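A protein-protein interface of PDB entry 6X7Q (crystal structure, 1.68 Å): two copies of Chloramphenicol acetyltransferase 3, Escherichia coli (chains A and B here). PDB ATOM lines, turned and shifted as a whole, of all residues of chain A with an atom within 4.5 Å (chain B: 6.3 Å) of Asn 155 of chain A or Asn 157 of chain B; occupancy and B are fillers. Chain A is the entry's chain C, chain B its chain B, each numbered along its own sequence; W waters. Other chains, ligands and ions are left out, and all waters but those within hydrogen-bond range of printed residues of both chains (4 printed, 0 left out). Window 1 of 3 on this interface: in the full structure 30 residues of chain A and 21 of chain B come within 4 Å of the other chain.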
ATOM      1  N   PRO A  27     -28.082  -7.034  25.060  1.00  0.00           N
ATOM      2  CA  PRO A  27     -27.511  -8.157  25.810  1.00  0.00           C
ATOM      3  C   PRO A  27     -27.261  -9.371  24.917  1.00  0.00           C
ATOM      4  O   PRO A  27     -28.178  -9.848  24.244  1.00  0.00           O
ATOM      5  CB  PRO A  27     -28.554  -8.436  26.904  1.00  0.00           C
ATOM      6  CG  PRO A  27     -29.394  -7.183  26.972  1.00  0.00           C
ATOM      7  CD  PRO A  27     -29.396  -6.618  25.583  1.00  0.00           C
ATOM      8  N   CYS A  28     -26.008  -9.805  24.861  1.00  0.00           N
ATOM      9  CA  CYS A  28     -25.671 -10.929  24.001  1.00  0.00           C
ATOM     10  C   CYS A  28     -24.319 -11.488  24.396  1.00  0.00           C
ATOM     11  O   CYS A  28     -23.540 -10.848  25.115  1.00  0.00           O
ATOM     12  CB  CYS A  28     -25.683 -10.569  22.527  1.00  0.00           C
ATOM     13  SG  CYS A  28     -24.384  -9.415  22.025  1.00  0.00           S
ATOM     14  N   GLY A  29     -24.118 -12.701  23.908  1.00  0.00           N
ATOM     15  CA  GLY A  29     -22.842 -13.367  23.932  1.00  0.00           C
ATOM     16  C   GLY A  29     -22.604 -14.089  22.609  1.00  0.00           C
ATOM     17  O   GLY A  29     -23.421 -14.009  21.705  1.00  0.00           O
ATOM     18  N   PHE A  30     -21.460 -14.738  22.495  1.00  0.00           N
ATOM     19  CA  PHE A  30     -21.151 -15.483  21.288  1.00  0.00           C
ATOM     20  C   PHE A  30     -20.395 -16.754  21.657  1.00  0.00           C
ATOM     21  O   PHE A  30     -19.751 -16.842  22.703  1.00  0.00           O
ATOM     22  CB  PHE A  30     -20.422 -14.658  20.222  1.00  0.00           C
ATOM     23  CG  PHE A  30     -19.101 -14.092  20.662  1.00  0.00           C
ATOM     24  CD1 PHE A  30     -19.037 -12.872  21.300  1.00  0.00           C
ATOM     25  CD2 PHE A  30     -17.913 -14.782  20.437  1.00  0.00           C
ATOM     26  CE1 PHE A  30     -17.831 -12.331  21.684  1.00  0.00           C
ATOM     27  CE2 PHE A  30     -16.697 -14.231  20.843  1.00  0.00           C
ATOM     28  CZ  PHE A  30     -16.662 -13.013  21.468  1.00  0.00           C
ATOM     29  N   SER A  31     -20.536 -17.758  20.782  1.00  0.00           N
ATOM     30  CA  SER A  31     -19.657 -18.910  20.787  1.00  0.00           C
ATOM     31  C   SER A  31     -18.824 -18.933  19.519  1.00  0.00           C
ATOM     32  O   SER A  31     -19.241 -18.479  18.441  1.00  0.00           O
ATOM     33  CB  SER A  31     -20.412 -20.227  20.913  1.00  0.00           C
ATOM     34  OG  SER A  31     -21.259 -20.426  19.773  1.00  0.00           O
ATOM     35  N   PHE A 154     -20.088 -26.162  18.217  1.00  0.00           N
ATOM     36  CA  PHE A 154     -20.877 -26.439  19.391  1.00  0.00           C
ATOM     37  C   PHE A 154     -21.347 -25.106  19.958  1.00  0.00           C
ATOM     38  O   PHE A 154     -20.539 -24.166  20.054  1.00  0.00           O
ATOM     39  CB  PHE A 154     -20.013 -27.237  20.378  1.00  0.00           C
ATOM     40  CG  PHE A 154     -20.727 -27.667  21.627  1.00  0.00           C
ATOM     41  CD1 PHE A 154     -20.818 -26.790  22.718  1.00  0.00           C
ATOM     42  CD2 PHE A 154     -21.385 -28.884  21.678  1.00  0.00           C
ATOM     43  CE1 PHE A 154     -21.518 -27.168  23.853  1.00  0.00           C
ATOM     44  CE2 PHE A 154     -22.036 -29.284  22.843  1.00  0.00           C
ATOM     45  CZ  PHE A 154     -22.129 -28.410  23.903  1.00  0.00           C
ATOM     46  N   ASN A 155     -22.641 -25.003  20.268  1.00  0.00           N
ATOM     47  CA  ASN A 155     -23.192 -23.785  20.837  1.00  0.00           C
ATOM     48  C   ASN A 155     -24.220 -24.188  21.882  1.00  0.00           C
ATOM     49  O   ASN A 155     -25.073 -25.041  21.604  1.00  0.00           O
ATOM     50  CB  ASN A 155     -23.937 -22.940  19.777  1.00  0.00           C
ATOM     51  CG  ASN A 155     -24.580 -21.680  20.329  1.00  0.00           C
ATOM     52  OD1 ASN A 155     -25.812 -21.551  20.522  1.00  0.00           O
ATOM     53  ND2 ASN A 155     -23.733 -20.718  20.583  1.00  0.00           N
ATOM     54  N   LEU A 156     -24.173 -23.514  23.032  1.00  0.00           N
ATOM     55  CA  LEU A 156     -25.191 -23.652  24.074  1.00  0.00           C
ATOM     56  C   LEU A 156     -26.235 -22.556  23.886  1.00  0.00           C
ATOM     57  O   LEU A 156     -25.910 -21.350  23.856  1.00  0.00           O
ATOM     58  CB  LEU A 156     -24.526 -23.553  25.453  1.00  0.00           C
ATOM     59  CG  LEU A 156     -23.732 -24.800  25.863  1.00  0.00           C
ATOM     60  CD1 LEU A 156     -22.641 -24.435  26.836  1.00  0.00           C
ATOM     61  CD2 LEU A 156     -24.639 -25.908  26.430  1.00  0.00           C
ATOM     62  N   ASN A 157     -27.482 -23.007  23.807  1.00  0.00           N
ATOM     63  CA  ASN A 157     -28.641 -22.147  23.745  1.00  0.00           C
ATOM     64  C   ASN A 157     -29.196 -22.057  25.164  1.00  0.00           C
ATOM     65  O   ASN A 157     -29.906 -22.968  25.590  1.00  0.00           O
ATOM     66  CB  ASN A 157     -29.648 -22.712  22.743  1.00  0.00           C
ATOM     67  CG  ASN A 157     -29.067 -22.751  21.343  1.00  0.00           C
ATOM     68  OD1 ASN A 157     -28.997 -23.825  20.721  1.00  0.00           O
ATOM     69  ND2 ASN A 157     -28.608 -21.609  20.872  1.00  0.00           N
ATOM     70  N   PHE A 161     -29.075 -16.007  30.293  1.00  0.00           N
ATOM     71  CA  PHE A 161     -27.650 -15.925  30.614  1.00  0.00           C
ATOM     72  C   PHE A 161     -27.282 -14.576  31.254  1.00  0.00           C
ATOM     73  O   PHE A 161     -26.085 -14.232  31.300  1.00  0.00           O
ATOM     74  CB  PHE A 161     -26.819 -16.195  29.346  1.00  0.00           C
ATOM     75  CG  PHE A 161     -27.075 -15.272  28.176  1.00  0.00           C
ATOM     76  CD1 PHE A 161     -26.519 -13.988  28.129  1.00  0.00           C
ATOM     77  CD2 PHE A 161     -27.742 -15.730  27.054  1.00  0.00           C
ATOM     78  CE1 PHE A 161     -26.764 -13.144  27.050  1.00  0.00           C
ATOM     79  CE2 PHE A 161     -27.970 -14.896  25.959  1.00  0.00           C
ATOM     80  CZ  PHE A 161     -27.485 -13.605  25.965  1.00  0.00           C
ATOM     81  N   GLN A 188     -17.397 -20.042  24.711  1.00  0.00           N
ATOM     82  CA  GLN A 188     -18.640 -19.301  24.681  1.00  0.00           C
ATOM     83  C   GLN A 188     -18.592 -18.283  25.807  1.00  0.00           C
ATOM     84  O   GLN A 188     -18.327 -18.645  26.970  1.00  0.00           O
ATOM     85  CB  GLN A 188     -19.824 -20.254  24.822  1.00  0.00           C
ATOM     86  CG  GLN A 188     -21.159 -19.561  24.813  1.00  0.00           C
ATOM     87  CD  GLN A 188     -22.298 -20.486  24.442  1.00  0.00           C
ATOM     88  OE1 GLN A 188     -22.110 -21.487  23.768  1.00  0.00           O
ATOM     89  NE2 GLN A 188     -23.495 -20.126  24.878  1.00  0.00           N
ATOM     90  N   ASN B 155     -21.571 -18.097  16.471  1.00  0.00           N
ATOM     91  CA  ASN B 155     -22.991 -17.855  16.679  1.00  0.00           C
ATOM     92  C   ASN B 155     -23.167 -16.781  17.735  1.00  0.00           C
ATOM     93  O   ASN B 155     -22.526 -16.856  18.778  1.00  0.00           O
ATOM     94  CB  ASN B 155     -23.752 -19.089  17.190  1.00  0.00           C
ATOM     95  CG  ASN B 155     -25.232 -18.883  17.456  1.00  0.00           C
ATOM     96  OD1 ASN B 155     -25.707 -18.774  18.628  1.00  0.00           O
ATOM     97  ND2 ASN B 155     -25.978 -18.761  16.384  1.00  0.00           N
ATOM     98  N   LEU B 156     -24.030 -15.798  17.455  1.00  0.00           N
ATOM     99  CA  LEU B 156     -24.406 -14.829  18.470  1.00  0.00           C
ATOM    100  C   LEU B 156     -25.654 -15.299  19.204  1.00  0.00           C
ATOM    101  O   LEU B 156     -26.671 -15.604  18.587  1.00  0.00           O
ATOM    102  CB  LEU B 156     -24.649 -13.497  17.763  1.00  0.00           C
ATOM    103  CG  LEU B 156     -23.369 -12.745  17.420  1.00  0.00           C
ATOM    104  CD1 LEU B 156     -23.688 -11.828  16.246  1.00  0.00           C
ATOM    105  CD2 LEU B 156     -22.826 -11.991  18.634  1.00  0.00           C
ATOM    106  N   ASN B 157     -25.559 -15.288  20.538  1.00  0.00           N
ATOM    107  CA  ASN B 157     -26.670 -15.605  21.433  1.00  0.00           C
ATOM    108  C   ASN B 157     -27.255 -14.301  21.970  1.00  0.00           C
ATOM    109  O   ASN B 157     -26.642 -13.666  22.834  1.00  0.00           O
ATOM    110  CB  ASN B 157     -26.193 -16.536  22.565  1.00  0.00           C
ATOM    111  CG  ASN B 157     -25.605 -17.834  22.026  1.00  0.00           C
ATOM    112  OD1 ASN B 157     -24.444 -18.201  22.303  1.00  0.00           O
ATOM    113  ND2 ASN B 157     -26.445 -18.558  21.338  1.00  0.00           N
ATOM    114  N   VAL B 158     -28.342 -13.852  21.336  1.00  0.00           N
ATOM    115  CA  VAL B 158     -28.918 -12.539  21.559  1.00  0.00           C
ATOM    116  C   VAL B 158     -30.134 -12.759  22.451  1.00  0.00           C
ATOM    117  O   VAL B 158     -31.007 -13.568  22.115  1.00  0.00           O
ATOM    118  CB  VAL B 158     -29.272 -11.863  20.215  1.00  0.00           C
ATOM    119  CG1 VAL B 158     -29.951 -10.504  20.411  1.00  0.00           C
ATOM    120  CG2 VAL B 158     -28.070 -11.735  19.285  1.00  0.00           C
ATOM    121  N   ALA B 159     -30.182 -12.066  23.590  1.00  0.00           N
ATOM    122  CA  ALA B 159     -31.270 -12.289  24.542  1.00  0.00           C
ATOM    123  C   ALA B 159     -32.651 -11.919  23.980  1.00  0.00           C
ATOM    124  O   ALA B 159     -33.627 -12.656  24.222  1.00  0.00           O
ATOM    125  CB  ALA B 159     -30.984 -11.533  25.822  1.00  0.00           C
ATOM    126  N   GLN B 188     -25.994 -14.700  10.073  1.00  0.00           N
ATOM    127  CA  GLN B 188     -27.036 -14.903  11.056  1.00  0.00           C
ATOM    128  C   GLN B 188     -28.234 -14.033  10.682  1.00  0.00           C
ATOM    129  O   GLN B 188     -28.128 -12.809  10.555  1.00  0.00           O
ATOM    130  CB  GLN B 188     -26.466 -14.631  12.442  1.00  0.00           C
ATOM    131  CG  GLN B 188     -27.450 -14.839  13.550  1.00  0.00           C
ATOM    132  CD  GLN B 188     -26.811 -15.082  14.906  1.00  0.00           C
ATOM    133  OE1 GLN B 188     -25.654 -15.467  15.014  1.00  0.00           O
ATOM    134  NE2 GLN B 188     -27.589 -14.859  15.951  1.00  0.00           N
HETATM  135  O   HOH W   1     -26.975 -19.003  24.758  1.00  0.00           O
HETATM  136  O   HOH W   2     -29.119 -18.991  21.177  1.00  0.00           O
HETATM  137  O   HOH W   3     -30.747  -8.830  23.487  1.00  0.00           O
HETATM  138  O   HOH W   4     -22.890 -16.713  24.507  1.00  0.00           O
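Asn 155 of chain A touches Asn 157 of chain B, but with the chains exchanged Asn 157 of chain A does not touch Asn 155 of chain B (4.6 Å).
Leu 156 of chain A touches Asn 157 of chain B, but with the chains exchanged Asn 157 of chain A does not touch Leu 156 of chain B (6.7 Å).
Asn 157 of chain A touches its own counterpart, Asn 157 of chain B.
Gln 188 of chain A touches Asn 157 of chain B, but with the chains exchanged Asn 157 of chain A does not touch Gln 188 of chain B (8.4 Å).
Of the 16 pairs that touch across the chains among the printed residues, 2 have their exchanged pair printed and touching as well.
Water W2 lies within hydrogen-bond range of the side-chain amide nitrogen (ND2) of Asn 157 of chain A (2.7 Å) and the side-chain amide nitrogen (ND2) of Asn 157 of chain B (2.7 Å).
Water W1 lies within hydrogen-bond range of the backbone carbonyl oxygen of Leu 156 of chain A (2.7 Å) and the side-chain amide nitrogen of Asn 157 of chain B (3.5 Å).
Water W3 bridges the backbone carbonyl oxygen (O) of Pro 27 of chain A (2.9 Å) and the backbone NH (N) of Ala 159 of chain B (3.3 Å).
Water W4 lies within hydrogen-bond range of OD1 of Asn 157 of chain B, N of Phe 30 of chain A and NE2 of Gln 188 of chain A.
The side-chain amide nitrogen (NE2) of Gln 188 of chain B is in hydrogen-bond range of the backbone carbonyl oxygen (O) of Leu 156 of chain B, at 2.9 Å.
The side-chain amide oxygen (OD1) of Asn 155 of chain B lies within hydrogen-bond range of the side-chain amide nitrogen (ND2) of Asn 157 of chain B (2.8 Å).
The side-chain amide nitrogen of Asn 155 of chain A lies within hydrogen-bond range of the side-chain hydroxyl of Ser 31 of chain A (2.6 Å).
O of Leu 156 of chain A sits at hydrogen-bond distance from NE2 of Gln 188 of chain A, 2.9 Å away.
The side-chain amide oxygen (OD1) of Asn 155 of chain A sits at hydrogen-bond distance from the side-chain amide nitrogen (ND2) of Asn 157 of chain A (2.8 Å).
Of chain A, only Cys 28 (3.1 Å), Gly 29 (2.8 Å), Asn 155 (3.1 Å), Leu 156 (3.8 Å), Asn 157 (3.8 Å), Phe 161 (3.2 Å) and Gln 188 (3.4 Å) come within 4 Å of Asn 157 of chain B.
Of the printed residues of chain A, Ala 159 of chain B touches Pro 27 and Phe 161.
Of the printed residues of chain A, Val 158 of chain B touches Pro 27 and Cys 28.
Of the printed residues of chain B, Ser 31 of chain A touches Asn 155 (3.0 Å).
Printed residues of chain B within 4 Å of Gly 29 of chain A: Leu 156 (3.5 Å) and Asn 157 (2.8 Å).
Gln 188 of chain B touches none of the printed residues of chain A.
The nearest residue of chain A that does not touch Asn 157 of chain B is Ser 31 of chain A (4.2 Å).
The backbone NH (N) of Asn 157 of chain B sits at hydrogen-bond distance from the backbone carbonyl oxygen (O) of Gly 29 of chain A.
The side-chain amide oxygen (OD1) of Asn 157 of chain B sits at hydrogen-bond distance from the side-chain amide nitrogen (ND2) of Asn 155 of chain A (3.1 Å).
O of Asn 155 of chain B is in hydrogen-bond range of N of Ser 31 of chain A, at 3.0 Å.
OD1 of Asn 155 of chain B lies close to OD1 of Asn 155 of chain A (3.4 Å).
O of Pro 27 of chain A sits at hydrogen-bond distance from N of Ala 159 of chain B, 3.1 Å away.
OD1 of Asn 157 of chain B is in hydrogen-bond range of NE2 of Gln 188 of chain A, at 3.4 Å.
Printed residues of chain B that touch a printed residue of chain A: Asn 155, Leu 156, Asn 157, Val 158 and Ala 159.
Of the 11 printed residues of chain A, 10 touch a printed residue of chain B.
Among the printed residues, pairs that only touch across the chains: Cys 28 of chain A with Asn 157 of chain B (3.1 Å), Phe 30 of chain A with Asn 155 of chain B (3.2 Å), Phe 161 of chain A with Asn 157 of chain B (3.2 Å), Gly 29 of chain A with Leu 156 of chain B (3.5 Å), Asn 157 of chain A with Asn 157 of chain B (3.8 Å), Leu 156 of chain A with Asn 157 of chain B (3.8 Å), Pro 27 of chain A with Val 158 of chain B (3.9 Å), Phe 161 of chain A with Ala 159 of chain B (3.9 Å), Cys 28 of chain A with Val 158 of chain B (3.9 Å) and Phe 30 of chain A with Leu 156 of chain B (3.9 Å).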
